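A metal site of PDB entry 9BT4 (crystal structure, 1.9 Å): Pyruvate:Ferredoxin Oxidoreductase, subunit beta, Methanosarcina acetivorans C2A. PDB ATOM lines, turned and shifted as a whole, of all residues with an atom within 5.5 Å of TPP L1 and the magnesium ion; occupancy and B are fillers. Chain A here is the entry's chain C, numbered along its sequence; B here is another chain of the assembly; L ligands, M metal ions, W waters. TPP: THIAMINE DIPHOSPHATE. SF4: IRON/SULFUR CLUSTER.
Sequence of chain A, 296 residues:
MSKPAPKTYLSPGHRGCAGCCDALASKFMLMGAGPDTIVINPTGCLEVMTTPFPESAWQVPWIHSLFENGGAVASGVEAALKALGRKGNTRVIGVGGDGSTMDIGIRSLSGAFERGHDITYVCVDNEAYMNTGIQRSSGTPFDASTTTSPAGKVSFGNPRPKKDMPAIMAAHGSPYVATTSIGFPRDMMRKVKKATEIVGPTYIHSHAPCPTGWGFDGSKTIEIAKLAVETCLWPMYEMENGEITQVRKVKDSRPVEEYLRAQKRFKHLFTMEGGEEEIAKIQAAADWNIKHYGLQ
Within 4 Å of the magnesium ion: Asp 98, Asn 126 and Ala 128. The nearest printed residue that does not touch the magnesium ion is Tyr 129 (4.1 Å).
The side-chain amide oxygen (OD1) of Asn 126 binds the magnesium ion, at 2.0 Å. O of Ala 128 binds the magnesium ion, at 2.0 Å. The magnesium ion is bound by O2A of TPP L1, 2.0 Å away. The magnesium ion is bound by OD1 of Asp 98 (2.0 Å). An oxygen (O3B) of TPP L1 is bound to the magnesium ion. Water W1 binds the magnesium ion (2.4 Å).
Water W1 lies within hydrogen-bond range of O of Val 124 (2.7 Å), O2B of TPP L1 (2.8 Å) and ND2 of Asn 126 (3.1 Å). Water W4 lies within hydrogen-bond range of O of Thr 43, O1A of TPP L1 and N of Gly 97. Water W2 bridges an oxygen (O2B) of TPP L1 (2.8 Å) and the side-chain carboxylate (OD2) of Asp 22 (3.5 Å). Water W3 bridges a nitrogen (N4') of TPP L1 (2.8 Å) and the guanidinium group of Arg 117 of chain B (2.9 Å). Water W5 lies within hydrogen-bond range of OG1 of Thr 43 (2.8 Å) and N4' of TPP L1 (3.4 Å).
Thr 43 touches TPP L1 (CG2 to C2, 3.6 Å). Gly 44 touches TPP L1. Phe 67 of chain A touches TPP L1. OE2 of Glu 68 touches CM2 of TPP L1 (3.1 Å). Gly 97 touches TPP L1. CD1 of Ile 104 touches CM2 of TPP L1 (3.7 Å). CD1 of Tyr 129 touches O7 of TPP L1, 3.4 Å away. Thr 132 touches TPP L1. CE2 of Tyr 35 of chain B touches C6' of TPP L1, at 3.7 Å. O of Pro 36 of chain B touches CM4 of TPP L1, 3.0 Å away. Ile 37 of chain B touches TPP L1 (CG1 to C7', 3.5 Å). Gln 91 of chain B touches TPP L1. CD2 of Leu 95 of chain B touches CM2 of TPP L1 (3.9 Å). Hydrophobic or aromatic side chains within 4 Å of TPP L1: Phe 67 of chain A, Ile 104, Tyr 129, Met 130, Tyr 35 of chain B, Ile 37 of chain B and Leu 95 of chain B. Within 4 Å of TPP L1: Asp 22, Thr 43, Gly 44, Cys 45, Phe 67 of chain A, Glu 68, Gly 97, Asp 98, Gly 99, Ser 100, Ile 104, Asn 126, Ala 128, Tyr 129, Met 130, Asn 131, Thr 132, Tyr 35 of chain B, Pro 36 of chain B, Ile 37 of chain B, Glu 67 of chain B, Gln 91 of chain B and Leu 95 of chain B. The nearest printed residue that does not touch TPP L1 is Gly 92 of chain B (4.2 Å).
An oxygen (O2A) of TPP L1 sits close to the backbone NH of Asp 98. O2B of TPP L1 lies close to OD2 of Asp 22, 2.6 Å away. N1' of TPP L1 sits at hydrogen-bond distance from OE1 of Glu 67 of chain B. An oxygen (O1A) of TPP L1 lies within hydrogen-bond range of the backbone NH (N) of Ser 100, 2.9 Å away. The backbone NH (N) of Cys 45 is in hydrogen-bond range of an oxygen (O1B) of TPP L1, at 3.0 Å. An oxygen (O1B) of TPP L1 lies close to the side-chain sulfur of Cys 45 (3.6 Å). The backbone NH (N) of Gly 99 lies within hydrogen-bond range of an oxygen (O1A) of TPP L1 (3.4 Å). N of Met 130 lies close to O3B of TPP L1. The backbone NH (N) of Asn 131 sits at hydrogen-bond distance from an oxygen (O1B) of TPP L1 (3.0 Å). ND2 of Asn 126 sits close to S1 of SF4 L2 (3.6 Å). SG of Cys 45 is bound to FE3 of SF4 L2, at 2.3 Å.
The side-chain amide nitrogen of Asn 126 lies within hydrogen-bond range of the side-chain carboxylate of Asp 22, at 3.3 Å. The backbone NH of Glu 127 sits at hydrogen-bond distance from the side-chain carboxylate of Asp 98. The backbone NH of Asp 98 lies within hydrogen-bond range of the backbone carbonyl oxygen of Val 124 (3.2 Å). OD2 of Asp 22 lies within hydrogen-bond range of N of Leu 46. OG of Ser 100 is in hydrogen-bond range of O of Phe 67 of chain A (2.7 Å). The backbone carbonyl oxygen of Gly 99 lies within hydrogen-bond range of the backbone NH of Ile 104, 3.2 Å away. OH of Tyr 35 of chain B sits at hydrogen-bond distance from OH of Tyr 129, 2.8 Å away. The backbone NH (N) of Tyr 129 sits at hydrogen-bond distance from the backbone carbonyl oxygen (O) of Gln 135, at 2.9 Å.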
ATOM      1  N   ASP A  22     -10.898  -0.902 -12.599  1.00  0.00           N
ATOM      2  CA  ASP A  22      -9.837   0.092 -12.516  1.00  0.00           C
ATOM      3  C   ASP A  22      -8.951  -0.194 -11.305  1.00  0.00           C
ATOM      4  O   ASP A  22      -7.738   0.024 -11.371  1.00  0.00           O
ATOM      5  CB  ASP A  22     -10.381   1.518 -12.483  1.00  0.00           C
ATOM      6  CG  ASP A  22     -10.813   2.108 -13.823  1.00  0.00           C
ATOM      7  OD1 ASP A  22     -11.000   1.338 -14.782  1.00  0.00           O
ATOM      8  OD2 ASP A  22     -10.937   3.342 -13.898  1.00  0.00           O
ATOM      9  N   THR A  43      -7.335  12.283 -15.109  1.00  0.00           N
ATOM     10  CA  THR A  43      -8.671  12.269 -14.545  1.00  0.00           C
ATOM     11  C   THR A  43      -9.448  11.041 -15.040  1.00  0.00           C
ATOM     12  O   THR A  43      -9.349  10.649 -16.200  1.00  0.00           O
ATOM     13  CB  THR A  43      -9.399  13.569 -14.911  1.00  0.00           C
ATOM     14  OG1 THR A  43      -8.490  14.634 -14.699  1.00  0.00           O
ATOM     15  CG2 THR A  43     -10.664  13.776 -14.095  1.00  0.00           C
ATOM     16  N   GLY A  44     -10.225  10.460 -14.133  1.00  0.00           N
ATOM     17  CA  GLY A  44     -11.047   9.307 -14.422  1.00  0.00           C
ATOM     18  C   GLY A  44     -11.427   8.606 -13.120  1.00  0.00           C
ATOM     19  O   GLY A  44     -11.088   9.087 -12.035  1.00  0.00           O
ATOM     20  N   CYS A  45     -12.123   7.475 -13.237  1.00  0.00           N
ATOM     21  CA  CYS A  45     -12.559   6.703 -12.082  1.00  0.00           C
ATOM     22  C   CYS A  45     -11.383   6.411 -11.166  1.00  0.00           C
ATOM     23  O   CYS A  45     -11.481   6.654  -9.967  1.00  0.00           O
ATOM     24  CB  CYS A  45     -13.172   5.394 -12.568  1.00  0.00           C
ATOM     25  SG  CYS A  45     -14.956   5.446 -12.876  1.00  0.00           S
ATOM     26  N   LEU A  46     -10.286   5.909 -11.736  1.00  0.00           N
ATOM     27  CA  LEU A  46      -9.131   5.487 -10.950  1.00  0.00           C
ATOM     28  C   LEU A  46      -8.649   6.648 -10.065  1.00  0.00           C
ATOM     29  O   LEU A  46      -8.480   6.474  -8.861  1.00  0.00           O
ATOM     30  CB  LEU A  46      -8.023   4.956 -11.856  1.00  0.00           C
ATOM     31  CG  LEU A  46      -6.720   4.548 -11.159  1.00  0.00           C
ATOM     32  CD1 LEU A  46      -6.947   3.465 -10.118  1.00  0.00           C
ATOM     33  CD2 LEU A  46      -5.686   4.100 -12.178  1.00  0.00           C
ATOM     34  N   PHE A  67      -6.984  15.893 -17.428  1.00  0.00           N
ATOM     35  CA  PHE A  67      -7.490  14.735 -18.138  1.00  0.00           C
ATOM     36  C   PHE A  67      -6.644  14.457 -19.385  1.00  0.00           C
ATOM     37  O   PHE A  67      -6.505  13.300 -19.792  1.00  0.00           O
ATOM     38  CB  PHE A  67      -8.963  15.005 -18.470  1.00  0.00           C
ATOM     39  CG  PHE A  67      -9.765  13.850 -19.065  1.00  0.00           C
ATOM     40  CD1 PHE A  67      -9.460  12.532 -18.757  1.00  0.00           C
ATOM     41  CD2 PHE A  67     -10.839  14.092 -19.915  1.00  0.00           C
ATOM     42  CE1 PHE A  67     -10.189  11.481 -19.302  1.00  0.00           C
ATOM     43  CE2 PHE A  67     -11.568  13.042 -20.460  1.00  0.00           C
ATOM     44  CZ  PHE A  67     -11.247  11.742 -20.150  1.00  0.00           C
ATOM     45  N   GLU A  68      -6.065  15.520 -19.976  1.00  0.00           N
ATOM     46  CA  GLU A  68      -5.496  15.415 -21.321  1.00  0.00           C
ATOM     47  C   GLU A  68      -3.975  15.206 -21.310  1.00  0.00           C
ATOM     48  O   GLU A  68      -3.404  14.887 -22.349  1.00  0.00           O
ATOM     49  CB  GLU A  68      -5.781  16.652 -22.172  1.00  0.00           C
ATOM     50  CG  GLU A  68      -7.155  17.287 -21.960  1.00  0.00           C
ATOM     51  CD  GLU A  68      -7.243  18.441 -20.968  1.00  0.00           C
ATOM     52  OE1 GLU A  68      -6.658  18.354 -19.866  1.00  0.00           O
ATOM     53  OE2 GLU A  68      -7.910  19.439 -21.298  1.00  0.00           O
ATOM     54  N   GLY A  96      -3.924   5.560 -17.253  1.00  0.00           N
ATOM     55  CA  GLY A  96      -5.109   6.308 -17.619  1.00  0.00           C
ATOM     56  C   GLY A  96      -6.132   5.416 -18.307  1.00  0.00           C
ATOM     57  O   GLY A  96      -5.804   4.351 -18.810  1.00  0.00           O
ATOM     58  N   GLY A  97      -7.385   5.878 -18.338  1.00  0.00           N
ATOM     59  CA  GLY A  97      -8.455   5.147 -19.005  1.00  0.00           C
ATOM     60  C   GLY A  97      -8.383   5.294 -20.523  1.00  0.00           C
ATOM     61  O   GLY A  97      -7.580   6.072 -21.046  1.00  0.00           O
ATOM     62  N   ASP A  98      -9.243   4.539 -21.212  1.00  0.00           N
ATOM     63  CA  ASP A  98      -9.399   4.565 -22.647  1.00  0.00           C
ATOM     64  C   ASP A  98      -9.638   5.995 -23.137  1.00  0.00           C
ATOM     65  O   ASP A  98      -9.024   6.450 -24.096  1.00  0.00           O
ATOM     66  CB  ASP A  98     -10.472   3.573 -23.084  1.00  0.00           C
ATOM     67  CG  ASP A  98     -11.791   3.670 -22.320  1.00  0.00           C
ATOM     68  OD1 ASP A  98     -11.805   3.465 -21.078  1.00  0.00           O
ATOM     69  OD2 ASP A  98     -12.810   3.971 -22.985  1.00  0.00           O
ATOM     70  N   GLY A  99     -10.535   6.712 -22.442  1.00  0.00           N
ATOM     71  CA  GLY A  99     -10.885   8.070 -22.827  1.00  0.00           C
ATOM     72  C   GLY A  99      -9.676   8.998 -22.752  1.00  0.00           C
ATOM     73  O   GLY A  99      -9.395   9.743 -23.697  1.00  0.00           O
ATOM     74  N   SER A 100      -8.952   8.922 -21.635  1.00  0.00           N
ATOM     75  CA  SER A 100      -7.778   9.744 -21.418  1.00  0.00           C
ATOM     76  C   SER A 100      -6.683   9.438 -22.436  1.00  0.00           C
ATOM     77  O   SER A 100      -6.007  10.348 -22.895  1.00  0.00           O
ATOM     78  CB  SER A 100      -7.261   9.599 -20.006  1.00  0.00           C
ATOM     79  OG  SER A 100      -6.336  10.641 -19.747  1.00  0.00           O
ATOM     80  N   THR A 101      -6.516   8.148 -22.767  1.00  0.00           N
ATOM     81  CA  THR A 101      -5.393   7.696 -23.575  1.00  0.00           C
ATOM     82  C   THR A 101      -5.696   7.909 -25.058  1.00  0.00           C
ATOM     83  O   THR A 101      -4.882   8.458 -25.802  1.00  0.00           O
ATOM     84  CB  THR A 101      -5.122   6.222 -23.297  1.00  0.00           C
ATOM     85  OG1 THR A 101      -4.842   6.123 -21.901  1.00  0.00           O
ATOM     86  CG2 THR A 101      -3.975   5.670 -24.115  1.00  0.00           C
ATOM     87  N   ILE A 104      -8.693  12.181 -25.577  1.00  0.00           N
ATOM     88  CA  ILE A 104      -8.356  13.560 -25.240  1.00  0.00           C
ATOM     89  C   ILE A 104      -6.860  13.708 -24.954  1.00  0.00           C
ATOM     90  O   ILE A 104      -6.308  14.799 -25.048  1.00  0.00           O
ATOM     91  CB  ILE A 104      -9.251  14.082 -24.098  1.00  0.00           C
ATOM     92  CG1 ILE A 104      -9.308  15.614 -24.075  1.00  0.00           C
ATOM     93  CG2 ILE A 104      -8.843  13.479 -22.746  1.00  0.00           C
ATOM     94  CD1 ILE A 104     -10.407  16.183 -23.192  1.00  0.00           C
ATOM     95  N   VAL A 124      -5.989   1.671 -19.228  1.00  0.00           N
ATOM     96  CA  VAL A 124      -7.015   0.861 -18.590  1.00  0.00           C
ATOM     97  C   VAL A 124      -8.298   1.018 -19.403  1.00  0.00           C
ATOM     98  O   VAL A 124      -9.048   1.988 -19.218  1.00  0.00           O
ATOM     99  CB  VAL A 124      -7.221   1.243 -17.120  1.00  0.00           C
ATOM    100  CG1 VAL A 124      -8.300   0.388 -16.446  1.00  0.00           C
ATOM    101  CG2 VAL A 124      -5.923   1.176 -16.321  1.00  0.00           C
ATOM    102  N   ASP A 125      -8.559   0.052 -20.292  1.00  0.00           N
ATOM    103  CA  ASP A 125      -9.591   0.200 -21.300  1.00  0.00           C
ATOM    104  C   ASP A 125     -10.864  -0.503 -20.844  1.00  0.00           C
ATOM    105  O   ASP A 125     -10.993  -1.722 -20.995  1.00  0.00           O
ATOM    106  CB  ASP A 125      -9.108  -0.320 -22.651  1.00  0.00           C
ATOM    107  CG  ASP A 125     -10.078  -0.150 -23.815  1.00  0.00           C
ATOM    108  OD1 ASP A 125     -11.194   0.401 -23.595  1.00  0.00           O
ATOM    109  OD2 ASP A 125      -9.725  -0.567 -24.943  1.00  0.00           O
ATOM    110  N   ASN A 126     -11.820   0.286 -20.325  1.00  0.00           N
ATOM    111  CA  ASN A 126     -13.142  -0.210 -19.973  1.00  0.00           C
ATOM    112  C   ASN A 126     -14.176   0.232 -21.014  1.00  0.00           C
ATOM    113  O   ASN A 126     -15.379   0.172 -20.744  1.00  0.00           O
ATOM    114  CB  ASN A 126     -13.505   0.132 -18.538  1.00  0.00           C
ATOM    115  CG  ASN A 126     -13.493   1.623 -18.259  1.00  0.00           C
ATOM    116  OD1 ASN A 126     -13.596   2.441 -19.177  1.00  0.00           O
ATOM    117  ND2 ASN A 126     -13.377   1.989 -16.990  1.00  0.00           N
ATOM    118  N   GLU A 127     -13.713   0.694 -22.179  1.00  0.00           N
ATOM    119  CA  GLU A 127     -14.526   0.833 -23.387  1.00  0.00           C
ATOM    120  C   GLU A 127     -15.633   1.870 -23.234  1.00  0.00           C
ATOM    121  O   GLU A 127     -16.654   1.796 -23.928  1.00  0.00           O
ATOM    122  CB  GLU A 127     -15.052  -0.545 -23.809  1.00  0.00           C
ATOM    123  CG  GLU A 127     -13.923  -1.509 -24.198  1.00  0.00           C
ATOM    124  CD  GLU A 127     -14.309  -2.800 -24.890  1.00  0.00           C
ATOM    125  OE1 GLU A 127     -15.495  -3.216 -24.836  1.00  0.00           O
ATOM    126  OE2 GLU A 127     -13.406  -3.391 -25.518  1.00  0.00           O
ATOM    127  N   ALA A 128     -15.421   2.844 -22.335  1.00  0.00           N
ATOM    128  CA  ALA A 128     -16.287   4.001 -22.193  1.00  0.00           C
ATOM    129  C   ALA A 128     -15.678   4.974 -21.193  1.00  0.00           C
ATOM    130  O   ALA A 128     -14.696   4.649 -20.513  1.00  0.00           O
ATOM    131  CB  ALA A 128     -17.695   3.597 -21.772  1.00  0.00           C
ATOM    132  N   TYR A 129     -16.252   6.179 -21.147  1.00  0.00           N
ATOM    133  CA  TYR A 129     -15.962   7.159 -20.104  1.00  0.00           C
ATOM    134  C   TYR A 129     -16.833   6.832 -18.900  1.00  0.00           C
ATOM    135  O   TYR A 129     -18.019   7.158 -18.887  1.00  0.00           O
ATOM    136  CB  TYR A 129     -16.285   8.584 -20.585  1.00  0.00           C
ATOM    137  CG  TYR A 129     -15.516   9.104 -21.790  1.00  0.00           C
ATOM    138  CD1 TYR A 129     -14.167   9.417 -21.707  1.00  0.00           C
ATOM    139  CD2 TYR A 129     -16.163   9.354 -23.001  1.00  0.00           C
ATOM    140  CE1 TYR A 129     -13.462   9.915 -22.793  1.00  0.00           C
ATOM    141  CE2 TYR A 129     -15.470   9.847 -24.092  1.00  0.00           C
ATOM    142  CZ  TYR A 129     -14.120  10.126 -23.995  1.00  0.00           C
ATOM    143  OH  TYR A 129     -13.436  10.624 -25.072  1.00  0.00           O
ATOM    144  N   MET A 130     -16.237   6.199 -17.872  1.00  0.00           N
ATOM    145  CA  MET A 130     -17.035   5.666 -16.785  1.00  0.00           C
ATOM    146  C   MET A 130     -17.308   6.709 -15.709  1.00  0.00           C
ATOM    147  O   MET A 130     -18.444   6.827 -15.250  1.00  0.00           O
ATOM    148  CB  MET A 130     -16.451   4.379 -16.183  1.00  0.00           C
ATOM    149  CG  MET A 130     -16.439   3.207 -17.148  1.00  0.00           C
ATOM    150  SD  MET A 130     -18.001   3.006 -18.019  1.00  0.00           S
ATOM    151  CE  MET A 130     -17.752   1.448 -18.882  1.00  0.00           C
ATOM    152  N   ASN A 131     -16.278   7.478 -15.308  1.00  0.00           N
ATOM    153  CA  ASN A 131     -16.430   8.389 -14.180  1.00  0.00           C
ATOM    154  C   ASN A 131     -17.591   9.355 -14.420  1.00  0.00           C
ATOM    155  O   ASN A 131     -18.285   9.728 -13.483  1.00  0.00           O
ATOM    156  CB  ASN A 131     -15.162   9.164 -13.860  1.00  0.00           C
ATOM    157  CG  ASN A 131     -15.244   9.816 -12.502  1.00  0.00           C
ATOM    158  OD1 ASN A 131     -15.171   9.136 -11.480  1.00  0.00           O
ATOM    159  ND2 ASN A 131     -15.402  11.137 -12.469  1.00  0.00           N
ATOM    160  N   THR A 132     -17.786   9.739 -15.687  1.00  0.00           N
ATOM    161  CA  THR A 132     -18.780  10.729 -16.079  1.00  0.00           C
ATOM    162  C   THR A 132     -20.143  10.089 -16.353  1.00  0.00           C
ATOM    163  O   THR A 132     -21.120  10.817 -16.560  1.00  0.00           O
ATOM    164  CB  THR A 132     -18.294  11.536 -17.289  1.00  0.00           C
ATOM    165  OG1 THR A 132     -17.667  10.581 -18.155  1.00  0.00           O
ATOM    166  CG2 THR A 132     -17.319  12.625 -16.900  1.00  0.00           C
ATOM    167  N   GLN A 135     -20.166   7.193 -21.146  1.00  0.00           N
ATOM    168  CA  GLN A 135     -20.343   7.796 -22.454  1.00  0.00           C
ATOM    169  C   GLN A 135     -19.370   7.167 -23.450  1.00  0.00           C
ATOM    170  O   GLN A 135     -18.345   6.621 -23.054  1.00  0.00           O
ATOM    171  CB  GLN A 135     -20.226   9.323 -22.446  1.00  0.00           C
ATOM    172  CG  GLN A 135     -21.286  10.035 -21.612  1.00  0.00           C
ATOM    173  CD  GLN A 135     -20.950  10.089 -20.138  1.00  0.00           C
ATOM    174  OE1 GLN A 135     -19.795   9.968 -19.734  1.00  0.00           O
ATOM    175  NE2 GLN A 135     -21.976  10.293 -19.315  1.00  0.00           N
ATOM    176  N   TYR B  35     -19.029  16.537 -25.969  1.00  0.00           N
ATOM    177  CA  TYR B  35     -17.997  15.896 -25.169  1.00  0.00           C
ATOM    178  C   TYR B  35     -18.483  15.837 -23.725  1.00  0.00           C
ATOM    179  O   TYR B  35     -18.942  16.837 -23.174  1.00  0.00           O
ATOM    180  CB  TYR B  35     -16.614  16.550 -25.357  1.00  0.00           C
ATOM    181  CG  TYR B  35     -15.513  15.603 -24.912  1.00  0.00           C
ATOM    182  CD1 TYR B  35     -15.120  14.551 -25.728  1.00  0.00           C
ATOM    183  CD2 TYR B  35     -14.906  15.725 -23.667  1.00  0.00           C
ATOM    184  CE1 TYR B  35     -14.144  13.650 -25.332  1.00  0.00           C
ATOM    185  CE2 TYR B  35     -13.928  14.827 -23.257  1.00  0.00           C
ATOM    186  CZ  TYR B  35     -13.541  13.793 -24.098  1.00  0.00           C
ATOM    187  OH  TYR B  35     -12.571  12.909 -23.727  1.00  0.00           O
ATOM    188  N   PRO B  36     -18.430  14.648 -23.065  1.00  0.00           N
ATOM    189  CA  PRO B  36     -18.995  14.505 -21.719  1.00  0.00           C
ATOM    190  C   PRO B  36     -18.117  15.091 -20.611  1.00  0.00           C
ATOM    191  O   PRO B  36     -16.893  14.978 -20.666  1.00  0.00           O
ATOM    192  CB  PRO B  36     -19.179  12.981 -21.568  1.00  0.00           C
ATOM    193  CG  PRO B  36     -18.095  12.397 -22.439  1.00  0.00           C
ATOM    194  CD  PRO B  36     -17.878  13.384 -23.576  1.00  0.00           C
ATOM    195  N   ILE B  37     -18.778  15.727 -19.639  1.00  0.00           N
ATOM    196  CA  ILE B  37     -18.159  16.188 -18.408  1.00  0.00           C
ATOM    197  C   ILE B  37     -19.267  16.484 -17.387  1.00  0.00           C
ATOM    198  O   ILE B  37     -20.225  17.181 -17.705  1.00  0.00           O
ATOM    199  CB  ILE B  37     -17.242  17.409 -18.643  1.00  0.00           C
ATOM    200  CG1 ILE B  37     -16.661  17.947 -17.323  1.00  0.00           C
ATOM    201  CG2 ILE B  37     -17.950  18.503 -19.439  1.00  0.00           C
ATOM    202  CD1 ILE B  37     -15.587  19.018 -17.498  1.00  0.00           C
ATOM    203  N   THR B  38     -19.120  15.933 -16.181  1.00  0.00           N
ATOM    204  CA  THR B  38     -20.018  16.187 -15.062  1.00  0.00           C
ATOM    205  C   THR B  38     -19.975  17.668 -14.725  1.00  0.00           C
ATOM    206  O   THR B  38     -18.885  18.249 -14.667  1.00  0.00           O
ATOM    207  CB  THR B  38     -19.560  15.338 -13.866  1.00  0.00           C
ATOM    208  OG1 THR B  38     -19.483  14.004 -14.331  1.00  0.00           O
ATOM    209  CG2 THR B  38     -20.506  15.412 -12.675  1.00  0.00           C
ATOM    210  N   GLU B  67     -13.182  18.665 -25.937  1.00  0.00           N
ATOM    211  CA  GLU B  67     -13.952  19.895 -26.009  1.00  0.00           C
ATOM    212  C   GLU B  67     -13.362  20.829 -27.067  1.00  0.00           C
ATOM    213  O   GLU B  67     -14.091  21.603 -27.685  1.00  0.00           O
ATOM    214  CB  GLU B  67     -14.008  20.680 -24.696  1.00  0.00           C
ATOM    215  CG  GLU B  67     -15.046  20.119 -23.718  1.00  0.00           C
ATOM    216  CD  GLU B  67     -14.539  19.003 -22.833  1.00  0.00           C
ATOM    217  OE1 GLU B  67     -13.366  18.570 -22.961  1.00  0.00           O
ATOM    218  OE2 GLU B  67     -15.346  18.576 -21.978  1.00  0.00           O
ATOM    219  N   GLN B  91     -13.660  22.190 -16.680  1.00  0.00           N
ATOM    220  CA  GLN B  91     -12.422  21.870 -17.367  1.00  0.00           C
ATOM    221  C   GLN B  91     -12.629  21.951 -18.882  1.00  0.00           C
ATOM    222  O   GLN B  91     -11.733  22.345 -19.615  1.00  0.00           O
ATOM    223  CB  GLN B  91     -11.920  20.467 -17.002  1.00  0.00           C
ATOM    224  CG  GLN B  91     -11.669  20.254 -15.515  1.00  0.00           C
ATOM    225  CD  GLN B  91     -10.809  21.314 -14.876  1.00  0.00           C
ATOM    226  OE1 GLN B  91      -9.742  21.698 -15.391  1.00  0.00           O
ATOM    227  NE2 GLN B  91     -11.258  21.832 -13.745  1.00  0.00           N
ATOM    228  N   GLY B  92     -13.825  21.556 -19.325  1.00  0.00           N
ATOM    229  CA  GLY B  92     -14.167  21.511 -20.734  1.00  0.00           C
ATOM    230  C   GLY B  92     -14.189  22.915 -21.341  1.00  0.00           C
ATOM    231  O   GLY B  92     -13.626  23.130 -22.419  1.00  0.00           O
ATOM    232  N   LEU B  95     -10.644  24.316 -21.563  1.00  0.00           N
ATOM    233  CA  LEU B  95      -9.902  23.805 -22.708  1.00  0.00           C
ATOM    234  C   LEU B  95     -10.305  24.597 -23.955  1.00  0.00           C
ATOM    235  O   LEU B  95      -9.467  24.839 -24.825  1.00  0.00           O
ATOM    236  CB  LEU B  95     -10.133  22.298 -22.862  1.00  0.00           C
ATOM    237  CG  LEU B  95      -9.515  21.615 -24.082  1.00  0.00           C
ATOM    238  CD1 LEU B  95      -8.010  21.803 -24.161  1.00  0.00           C
ATOM    239  CD2 LEU B  95      -9.891  20.134 -24.133  1.00  0.00           C
ATOM    240  N   ARG B 117     -19.528  24.662 -13.218  1.00  0.00           N
ATOM    241  CA  ARG B 117     -18.830  23.846 -12.240  1.00  0.00           C
ATOM    242  C   ARG B 117     -17.432  24.427 -11.987  1.00  0.00           C
ATOM    243  O   ARG B 117     -16.811  25.009 -12.879  1.00  0.00           O
ATOM    244  CB  ARG B 117     -18.744  22.399 -12.727  1.00  0.00           C
ATOM    245  CG  ARG B 117     -17.674  21.572 -12.036  1.00  0.00           C
ATOM    246  CD  ARG B 117     -17.377  20.278 -12.777  1.00  0.00           C
ATOM    247  NE  ARG B 117     -15.991  19.854 -12.528  1.00  0.00           N
ATOM    248  CZ  ARG B 117     -15.395  18.827 -13.100  1.00  0.00           C
ATOM    249  NH1 ARG B 117     -16.061  18.034 -13.915  1.00  0.00           N
ATOM    250  NH2 ARG B 117     -14.116  18.572 -12.832  1.00  0.00           N
ATOM    251  N   ILE B 123      -9.196  19.478  -8.325  1.00  0.00           N
ATOM    252  CA  ILE B 123     -10.381  19.089  -9.082  1.00  0.00           C
ATOM    253  C   ILE B 123     -11.576  18.972  -8.125  1.00  0.00           C
ATOM    254  O   ILE B 123     -11.442  18.529  -6.985  1.00  0.00           O
ATOM    255  CB  ILE B 123     -10.113  17.809  -9.890  1.00  0.00           C
ATOM    256  CG1 ILE B 123     -11.301  17.430 -10.794  1.00  0.00           C
ATOM    257  CG2 ILE B 123      -9.682  16.643  -8.987  1.00  0.00           C
ATOM    258  CD1 ILE B 123     -10.977  16.419 -11.866  1.00  0.00           C
HETATM  259  N1' TPP L   1     -12.856  17.391 -20.590  1.00  0.00           N
HETATM  260  C2' TPP L   1     -11.812  17.842 -19.898  1.00  0.00           C
HETATM  261  CM2 TPP L   1     -10.878  18.774 -20.603  1.00  0.00           C
HETATM  262  N3' TPP L   1     -11.538  17.516 -18.642  1.00  0.00           N
HETATM  263  C4' TPP L   1     -12.375  16.676 -18.009  1.00  0.00           C
HETATM  264  N4' TPP L   1     -12.088  16.358 -16.735  1.00  0.00           N
HETATM  265  C5' TPP L   1     -13.507  16.130 -18.666  1.00  0.00           C
HETATM  266  C6' TPP L   1     -13.704  16.551 -19.970  1.00  0.00           C
HETATM  267  C7' TPP L   1     -14.500  15.214 -17.994  1.00  0.00           C
HETATM  268  N3  TPP L   1     -13.997  13.890 -17.639  1.00  0.00           N
HETATM  269  C2  TPP L   1     -13.253  13.627 -16.528  1.00  0.00           C
HETATM  270  S1  TPP L   1     -12.920  11.985 -16.415  1.00  0.00           S
HETATM  271  C5  TPP L   1     -13.771  11.567 -17.793  1.00  0.00           C
HETATM  272  C4  TPP L   1     -14.322  12.710 -18.360  1.00  0.00           C
HETATM  273  CM4 TPP L   1     -15.156  12.742 -19.602  1.00  0.00           C
HETATM  274  C6  TPP L   1     -13.920  10.174 -18.290  1.00  0.00           C
HETATM  275  C7  TPP L   1     -12.761   9.303 -17.969  1.00  0.00           C
HETATM  276  O7  TPP L   1     -12.869   8.178 -18.875  1.00  0.00           O
HETATM  277  PA  TPP L   1     -11.622   7.194 -19.023  1.00  0.00           P
HETATM  278  O1A TPP L   1     -10.395   8.007 -19.289  1.00  0.00           O
HETATM  279  O2A TPP L   1     -12.042   6.070 -19.937  1.00  0.00           O
HETATM  280  O3A TPP L   1     -11.535   6.653 -17.524  1.00  0.00           O
HETATM  281  PB  TPP L   1     -12.602   5.753 -16.711  1.00  0.00           P
HETATM  282  O1B TPP L   1     -13.380   6.722 -15.834  1.00  0.00           O
HETATM  283  O2B TPP L   1     -11.761   4.798 -15.906  1.00  0.00           O
HETATM  284  O3B TPP L   1     -13.423   5.073 -17.797  1.00  0.00           O
HETATM  285 FE1  SF4 L   2     -17.220   1.667 -10.995  1.00  0.00          FE
HETATM  286 FE2  SF4 L   2     -14.623   1.000 -11.330  1.00  0.00          FE
HETATM  287 FE3  SF4 L   2     -15.603   3.311 -12.445  1.00  0.00          FE
HETATM  288 FE4  SF4 L   2     -16.323   0.876 -13.495  1.00  0.00          FE
HETATM  289  S1  SF4 L   2     -14.238   1.783 -13.455  1.00  0.00           S
HETATM  290  S2  SF4 L   2     -17.699   2.649 -12.986  1.00  0.00           S
HETATM  291  S3  SF4 L   2     -16.392  -0.379 -11.605  1.00  0.00           S
HETATM  292  S4  SF4 L   2     -15.412   2.826 -10.212  1.00  0.00           S
HETATM  293 MG    MG M   1     -12.937   4.287 -19.607  1.00  0.00          MG
HETATM  294  O   HOH W   1     -11.042   3.548 -18.322  1.00  0.00           O
HETATM  295  O   HOH W   2      -9.424   6.126 -15.288  1.00  0.00           O
HETATM  296  O   HOH W   3     -13.805  16.257 -14.470  1.00  0.00           O
HETATM  297  O   HOH W   4      -8.634   8.290 -17.242  1.00  0.00           O
HETATM  298  O   HOH W   5      -9.272  17.325 -14.997  1.00  0.00           O
